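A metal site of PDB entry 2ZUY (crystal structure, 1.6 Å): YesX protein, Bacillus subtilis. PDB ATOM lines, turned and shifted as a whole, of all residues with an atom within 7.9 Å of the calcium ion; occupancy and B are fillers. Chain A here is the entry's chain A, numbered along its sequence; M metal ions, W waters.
O of Phe 185 lies close to OD1 of Asn 576. The backbone NH (N) of Ala 578 lies within hydrogen-bond range of the side-chain amide oxygen (OE1) of Gln 184, at 2.8 Å. O of Asp 120 is in hydrogen-bond range of N of Lys 137. The side-chain amide nitrogen (ND2) of Asn 516 lies within hydrogen-bond range of the side-chain carboxylate (OD1) of Asp 120 (3.1 Å). OD1 of Asp 120 sits close to OD1 of Asn 119 (3.4 Å).
Within 4 Å of the calcium ion: Asp 120, Asn 576, Ala 578 and Asn 580. Along chain A the residues within 4 Å of the calcium ion span positions 120 to 580. The nearest printed residue that does not touch the calcium ion is Thr 577 (4.1 Å).
The calcium ion is bound by the backbone carbonyl oxygen of Asn 576, the backbone carbonyl oxygen of Ala 578, water W1, the side-chain amide oxygen of Asn 580, the side-chain carboxylate of Asp 120 and water W2. The calcium ion has six donor atoms within binding distance.
Water W2 lies within hydrogen-bond range of the backbone carbonyl oxygen of Ala 180, the side-chain amino group of Lys 137 and the backbone NH of Ala 578.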
ATOM      1  N   ASN A 119     -13.773   2.682 -16.643  1.00  0.00           N
ATOM      2  CA  ASN A 119     -13.237   3.890 -17.273  1.00  0.00           C
ATOM      3  C   ASN A 119     -13.336   3.771 -18.803  1.00  0.00           C
ATOM      4  O   ASN A 119     -14.364   3.296 -19.315  1.00  0.00           O
ATOM      5  CB  ASN A 119     -11.822   4.164 -16.737  1.00  0.00           C
ATOM      6  CG  ASN A 119     -11.348   5.598 -17.002  1.00  0.00           C
ATOM      7  OD1 ASN A 119     -10.563   5.826 -17.913  1.00  0.00           O
ATOM      8  ND2 ASN A 119     -11.803   6.555 -16.185  1.00  0.00           N
ATOM      9  N   ASP A 120     -12.303   4.191 -19.551  1.00  0.00           N
ATOM     10  CA  ASP A 120     -12.351   4.162 -21.015  1.00  0.00           C
ATOM     11  C   ASP A 120     -12.499   2.744 -21.546  1.00  0.00           C
ATOM     12  O   ASP A 120     -11.940   1.799 -20.978  1.00  0.00           O
ATOM     13  CB  ASP A 120     -11.069   4.709 -21.653  1.00  0.00           C
ATOM     14  CG  ASP A 120     -10.751   6.131 -21.243  1.00  0.00           C
ATOM     15  OD1 ASP A 120     -11.671   6.905 -20.908  1.00  0.00           O
ATOM     16  OD2 ASP A 120      -9.548   6.465 -21.300  1.00  0.00           O
ATOM     17  N   ALA A 121     -13.222   2.616 -22.659  1.00  0.00           N
ATOM     18  CA  ALA A 121     -13.312   1.327 -23.351  1.00  0.00           C
ATOM     19  C   ALA A 121     -12.988   1.462 -24.838  1.00  0.00           C
ATOM     20  O   ALA A 121     -12.889   2.559 -25.391  1.00  0.00           O
ATOM     21  CB  ALA A 121     -14.707   0.709 -23.173  1.00  0.00           C
ATOM     22  N   LYS A 137     -10.938  -0.522 -19.679  1.00  0.00           N
ATOM     23  CA  LYS A 137      -9.905  -0.098 -18.736  1.00  0.00           C
ATOM     24  C   LYS A 137     -10.523   0.288 -17.392  1.00  0.00           C
ATOM     25  O   LYS A 137     -11.465   1.079 -17.342  1.00  0.00           O
ATOM     26  CB  LYS A 137      -9.118   1.083 -19.315  1.00  0.00           C
ATOM     27  CG  LYS A 137      -7.930   1.555 -18.465  1.00  0.00           C
ATOM     28  CD  LYS A 137      -7.195   2.727 -19.136  1.00  0.00           C
ATOM     29  CE  LYS A 137      -7.924   4.044 -18.910  1.00  0.00           C
ATOM     30  NZ  LYS A 137      -7.350   5.165 -19.757  1.00  0.00           N
ATOM     31  N   GLY A 179      -3.279   6.797 -15.087  1.00  0.00           N
ATOM     32  CA  GLY A 179      -3.577   8.178 -15.433  1.00  0.00           C
ATOM     33  C   GLY A 179      -3.869   8.283 -16.923  1.00  0.00           C
ATOM     34  O   GLY A 179      -3.499   7.408 -17.713  1.00  0.00           O
ATOM     35  N   ALA A 180      -4.514   9.388 -17.304  1.00  0.00           N
ATOM     36  CA  ALA A 180      -4.978   9.571 -18.682  1.00  0.00           C
ATOM     37  C   ALA A 180      -3.876   9.427 -19.729  1.00  0.00           C
ATOM     38  O   ALA A 180      -4.099   8.904 -20.815  1.00  0.00           O
ATOM     39  CB  ALA A 180      -5.676  10.917 -18.835  1.00  0.00           C
ATOM     40  N   HIS A 181      -2.669   9.881 -19.375  1.00  0.00           N
ATOM     41  CA  HIS A 181      -1.602  10.007 -20.370  1.00  0.00           C
ATOM     42  C   HIS A 181      -0.677   8.817 -20.455  1.00  0.00           C
ATOM     43  O   HIS A 181       0.241   8.811 -21.290  1.00  0.00           O
ATOM     44  CB  HIS A 181      -0.810  11.291 -20.091  1.00  0.00           C
ATOM     45  CG  HIS A 181      -1.682  12.497 -20.070  1.00  0.00           C
ATOM     46  ND1 HIS A 181      -2.349  12.941 -21.199  1.00  0.00           N
ATOM     47  CD2 HIS A 181      -2.068  13.304 -19.067  1.00  0.00           C
ATOM     48  CE1 HIS A 181      -3.066  13.998 -20.892  1.00  0.00           C
ATOM     49  NE2 HIS A 181      -2.925  14.236 -19.595  1.00  0.00           N
ATOM     50  N   THR A 183      -1.327   4.540 -20.085  1.00  0.00           N
ATOM     51  CA  THR A 183      -1.784   3.449 -20.963  1.00  0.00           C
ATOM     52  C   THR A 183      -2.731   3.933 -22.051  1.00  0.00           C
ATOM     53  O   THR A 183      -3.744   4.585 -21.760  1.00  0.00           O
ATOM     54  CB  THR A 183      -2.490   2.329 -20.178  1.00  0.00           C
ATOM     55  OG1 THR A 183      -1.586   1.797 -19.204  1.00  0.00           O
ATOM     56  CG2 THR A 183      -2.946   1.194 -21.114  1.00  0.00           C
ATOM     57  N   GLN A 184      -2.385   3.614 -23.303  1.00  0.00           N
ATOM     58  CA  GLN A 184      -3.226   3.896 -24.470  1.00  0.00           C
ATOM     59  C   GLN A 184      -3.377   2.542 -25.146  1.00  0.00           C
ATOM     60  O   GLN A 184      -2.395   1.994 -25.660  1.00  0.00           O
ATOM     61  CB  GLN A 184      -2.533   4.898 -25.409  1.00  0.00           C
ATOM     62  CG  GLN A 184      -1.896   6.101 -24.709  1.00  0.00           C
ATOM     63  CD  GLN A 184      -2.875   6.908 -23.879  1.00  0.00           C
ATOM     64  OE1 GLN A 184      -4.068   6.935 -24.159  1.00  0.00           O
ATOM     65  NE2 GLN A 184      -2.362   7.567 -22.855  1.00  0.00           N
ATOM     66  N   PHE A 185      -4.575   1.983 -25.080  1.00  0.00           N
ATOM     67  CA  PHE A 185      -4.768   0.614 -25.550  1.00  0.00           C
ATOM     68  C   PHE A 185      -5.440   0.566 -26.918  1.00  0.00           C
ATOM     69  O   PHE A 185      -6.526   1.129 -27.116  1.00  0.00           O
ATOM     70  CB  PHE A 185      -5.465  -0.277 -24.500  1.00  0.00           C
ATOM     71  CG  PHE A 185      -6.835   0.197 -24.094  1.00  0.00           C
ATOM     72  CD1 PHE A 185      -6.990   1.273 -23.212  1.00  0.00           C
ATOM     73  CD2 PHE A 185      -7.974  -0.464 -24.560  1.00  0.00           C
ATOM     74  CE1 PHE A 185      -8.260   1.711 -22.826  1.00  0.00           C
ATOM     75  CE2 PHE A 185      -9.247  -0.034 -24.169  1.00  0.00           C
ATOM     76  CZ  PHE A 185      -9.390   1.053 -23.302  1.00  0.00           C
ATOM     77  N   HIS A 330      -3.718  16.355 -26.817  1.00  0.00           N
ATOM     78  CA  HIS A 330      -4.004  15.177 -25.990  1.00  0.00           C
ATOM     79  C   HIS A 330      -4.889  14.161 -26.735  1.00  0.00           C
ATOM     80  O   HIS A 330      -5.665  13.429 -26.121  1.00  0.00           O
ATOM     81  CB  HIS A 330      -4.719  15.562 -24.689  1.00  0.00           C
ATOM     82  CG  HIS A 330      -4.029  16.627 -23.878  1.00  0.00           C
ATOM     83  ND1 HIS A 330      -2.907  16.377 -23.116  1.00  0.00           N
ATOM     84  CD2 HIS A 330      -4.363  17.915 -23.660  1.00  0.00           C
ATOM     85  CE1 HIS A 330      -2.554  17.487 -22.489  1.00  0.00           C
ATOM     86  NE2 HIS A 330      -3.424  18.429 -22.790  1.00  0.00           N
ATOM     87  N   ASN A 516     -13.575  10.452 -15.891  1.00  0.00           N
ATOM     88  CA  ASN A 516     -12.398  11.312 -16.034  1.00  0.00           C
ATOM     89  C   ASN A 516     -12.616  12.746 -15.587  1.00  0.00           C
ATOM     90  O   ASN A 516     -12.148  13.709 -16.227  1.00  0.00           O
ATOM     91  CB  ASN A 516     -11.824  11.201 -17.455  1.00  0.00           C
ATOM     92  CG  ASN A 516     -11.383   9.779 -17.779  1.00  0.00           C
ATOM     93  OD1 ASN A 516     -10.716   9.127 -16.959  1.00  0.00           O
ATOM     94  ND2 ASN A 516     -11.758   9.285 -18.954  1.00  0.00           N
ATOM     95  N   ASN A 521     -16.326  11.981 -19.868  1.00  0.00           N
ATOM     96  CA  ASN A 521     -16.374  11.014 -20.945  1.00  0.00           C
ATOM     97  C   ASN A 521     -17.382   9.895 -20.702  1.00  0.00           C
ATOM     98  O   ASN A 521     -17.557   9.463 -19.565  1.00  0.00           O
ATOM     99  CB  ASN A 521     -15.011  10.327 -21.114  1.00  0.00           C
ATOM    100  CG  ASN A 521     -13.895  11.298 -21.401  1.00  0.00           C
ATOM    101  OD1 ASN A 521     -12.819  11.180 -20.820  1.00  0.00           O
ATOM    102  ND2 ASN A 521     -14.129  12.262 -22.303  1.00  0.00           N
ATOM    103  N   TRP A 574      -9.111   5.064 -31.559  1.00  0.00           N
ATOM    104  CA  TRP A 574      -8.403   6.034 -30.711  1.00  0.00           C
ATOM    105  C   TRP A 574      -9.244   6.783 -29.680  1.00  0.00           C
ATOM    106  O   TRP A 574      -8.739   7.670 -28.985  1.00  0.00           O
ATOM    107  CB  TRP A 574      -7.520   7.011 -31.528  1.00  0.00           C
ATOM    108  CG  TRP A 574      -8.139   7.787 -32.697  1.00  0.00           C
ATOM    109  CD1 TRP A 574      -7.774   7.667 -34.012  1.00  0.00           C
ATOM    110  CD2 TRP A 574      -9.141   8.836 -32.657  1.00  0.00           C
ATOM    111  NE1 TRP A 574      -8.500   8.542 -34.793  1.00  0.00           N
ATOM    112  CE2 TRP A 574      -9.330   9.280 -33.990  1.00  0.00           C
ATOM    113  CE3 TRP A 574      -9.883   9.438 -31.629  1.00  0.00           C
ATOM    114  CZ2 TRP A 574     -10.252  10.281 -34.328  1.00  0.00           C
ATOM    115  CZ3 TRP A 574     -10.803  10.447 -31.972  1.00  0.00           C
ATOM    116  CH2 TRP A 574     -10.977  10.845 -33.315  1.00  0.00           C
ATOM    117  N   GLN A 575     -10.528   6.438 -29.543  1.00  0.00           N
ATOM    118  CA  GLN A 575     -11.369   7.198 -28.621  1.00  0.00           C
ATOM    119  C   GLN A 575     -10.792   7.259 -27.206  1.00  0.00           C
ATOM    120  O   GLN A 575     -10.819   8.312 -26.561  1.00  0.00           O
ATOM    121  CB  GLN A 575     -12.798   6.660 -28.581  1.00  0.00           C
ATOM    122  CG  GLN A 575     -13.742   7.623 -27.859  1.00  0.00           C
ATOM    123  CD  GLN A 575     -15.187   7.292 -28.106  1.00  0.00           C
ATOM    124  OE1 GLN A 575     -15.646   7.272 -29.262  1.00  0.00           O
ATOM    125  NE2 GLN A 575     -15.911   6.995 -27.041  1.00  0.00           N
ATOM    126  N   ASN A 576     -10.254   6.136 -26.713  1.00  0.00           N
ATOM    127  CA  ASN A 576      -9.711   6.116 -25.357  1.00  0.00           C
ATOM    128  C   ASN A 576      -8.454   6.960 -25.175  1.00  0.00           C
ATOM    129  O   ASN A 576      -8.122   7.364 -24.060  1.00  0.00           O
ATOM    130  CB  ASN A 576      -9.447   4.672 -24.886  1.00  0.00           C
ATOM    131  CG  ASN A 576      -8.281   4.029 -25.601  1.00  0.00           C
ATOM    132  OD1 ASN A 576      -8.444   3.385 -26.650  1.00  0.00           O
ATOM    133  ND2 ASN A 576      -7.091   4.175 -25.034  1.00  0.00           N
ATOM    134  N   THR A 577      -7.756   7.219 -26.282  1.00  0.00           N
ATOM    135  CA  THR A 577      -6.436   7.858 -26.253  1.00  0.00           C
ATOM    136  C   THR A 577      -6.464   9.182 -25.490  1.00  0.00           C
ATOM    137  O   THR A 577      -7.206  10.097 -25.842  1.00  0.00           O
ATOM    138  CB  THR A 577      -5.888   8.062 -27.686  1.00  0.00           C
ATOM    139  OG1 THR A 577      -5.615   6.776 -28.263  1.00  0.00           O
ATOM    140  CG2 THR A 577      -4.619   8.881 -27.670  1.00  0.00           C
ATOM    141  N   ALA A 578      -5.628   9.260 -24.456  1.00  0.00           N
ATOM    142  CA  ALA A 578      -5.469  10.460 -23.600  1.00  0.00           C
ATOM    143  C   ALA A 578      -6.798  11.150 -23.317  1.00  0.00           C
ATOM    144  O   ALA A 578      -7.680  10.516 -22.746  1.00  0.00           O
ATOM    145  CB  ALA A 578      -4.423  11.417 -24.173  1.00  0.00           C
ATOM    146  N   TYR A 579      -6.954  12.417 -23.689  1.00  0.00           N
ATOM    147  CA  TYR A 579      -8.223  13.105 -23.414  1.00  0.00           C
ATOM    148  C   TYR A 579      -9.199  12.806 -24.548  1.00  0.00           C
ATOM    149  O   TYR A 579      -9.175  13.460 -25.602  1.00  0.00           O
ATOM    150  CB  TYR A 579      -8.036  14.619 -23.248  1.00  0.00           C
ATOM    151  CG  TYR A 579      -7.243  15.027 -22.039  1.00  0.00           C
ATOM    152  CD1 TYR A 579      -7.058  14.158 -20.954  1.00  0.00           C
ATOM    153  CD2 TYR A 579      -6.668  16.309 -21.969  1.00  0.00           C
ATOM    154  CE1 TYR A 579      -6.316  14.557 -19.838  1.00  0.00           C
ATOM    155  CE2 TYR A 579      -5.929  16.702 -20.865  1.00  0.00           C
ATOM    156  CZ  TYR A 579      -5.750  15.812 -19.801  1.00  0.00           C
ATOM    157  OH  TYR A 579      -5.015  16.190 -18.705  1.00  0.00           O
ATOM    158  N   ASN A 580     -10.022  11.789 -24.303  1.00  0.00           N
ATOM    159  CA  ASN A 580     -10.934  11.192 -25.304  1.00  0.00           C
ATOM    160  C   ASN A 580     -11.619  12.237 -26.185  1.00  0.00           C
ATOM    161  O   ASN A 580     -12.244  13.169 -25.675  1.00  0.00           O
ATOM    162  CB  ASN A 580     -12.058  10.389 -24.614  1.00  0.00           C
ATOM    163  CG  ASN A 580     -11.547   9.348 -23.623  1.00  0.00           C
ATOM    164  OD1 ASN A 580     -10.427   9.414 -23.117  1.00  0.00           O
ATOM    165  ND2 ASN A 580     -12.409   8.376 -23.323  1.00  0.00           N
ATOM    166  N   GLN A 581     -11.560  12.012 -27.500  1.00  0.00           N
ATOM    167  CA  GLN A 581     -12.217  12.870 -28.482  1.00  0.00           C
ATOM    168  C   GLN A 581     -13.254  12.060 -29.278  1.00  0.00           C
ATOM    169  O   GLN A 581     -13.111  10.851 -29.437  1.00  0.00           O
ATOM    170  CB  GLN A 581     -11.183  13.492 -29.428  1.00  0.00           C
ATOM    171  CG  GLN A 581     -10.236  14.466 -28.718  1.00  0.00           C
ATOM    172  CD  GLN A 581     -10.962  15.658 -28.111  1.00  0.00           C
ATOM    173  OE1 GLN A 581     -11.602  16.420 -28.823  1.00  0.00           O
ATOM    174  NE2 GLN A 581     -10.858  15.814 -26.791  1.00  0.00           N
HETATM  175 CA    CA M   1      -8.548   8.461 -22.065  1.00  0.00          CA
HETATM  176  O   HOH W   1      -8.474   9.292 -19.877  1.00  0.00           O
HETATM  177  O   HOH W   2      -6.422   7.544 -21.521  1.00  0.00           O
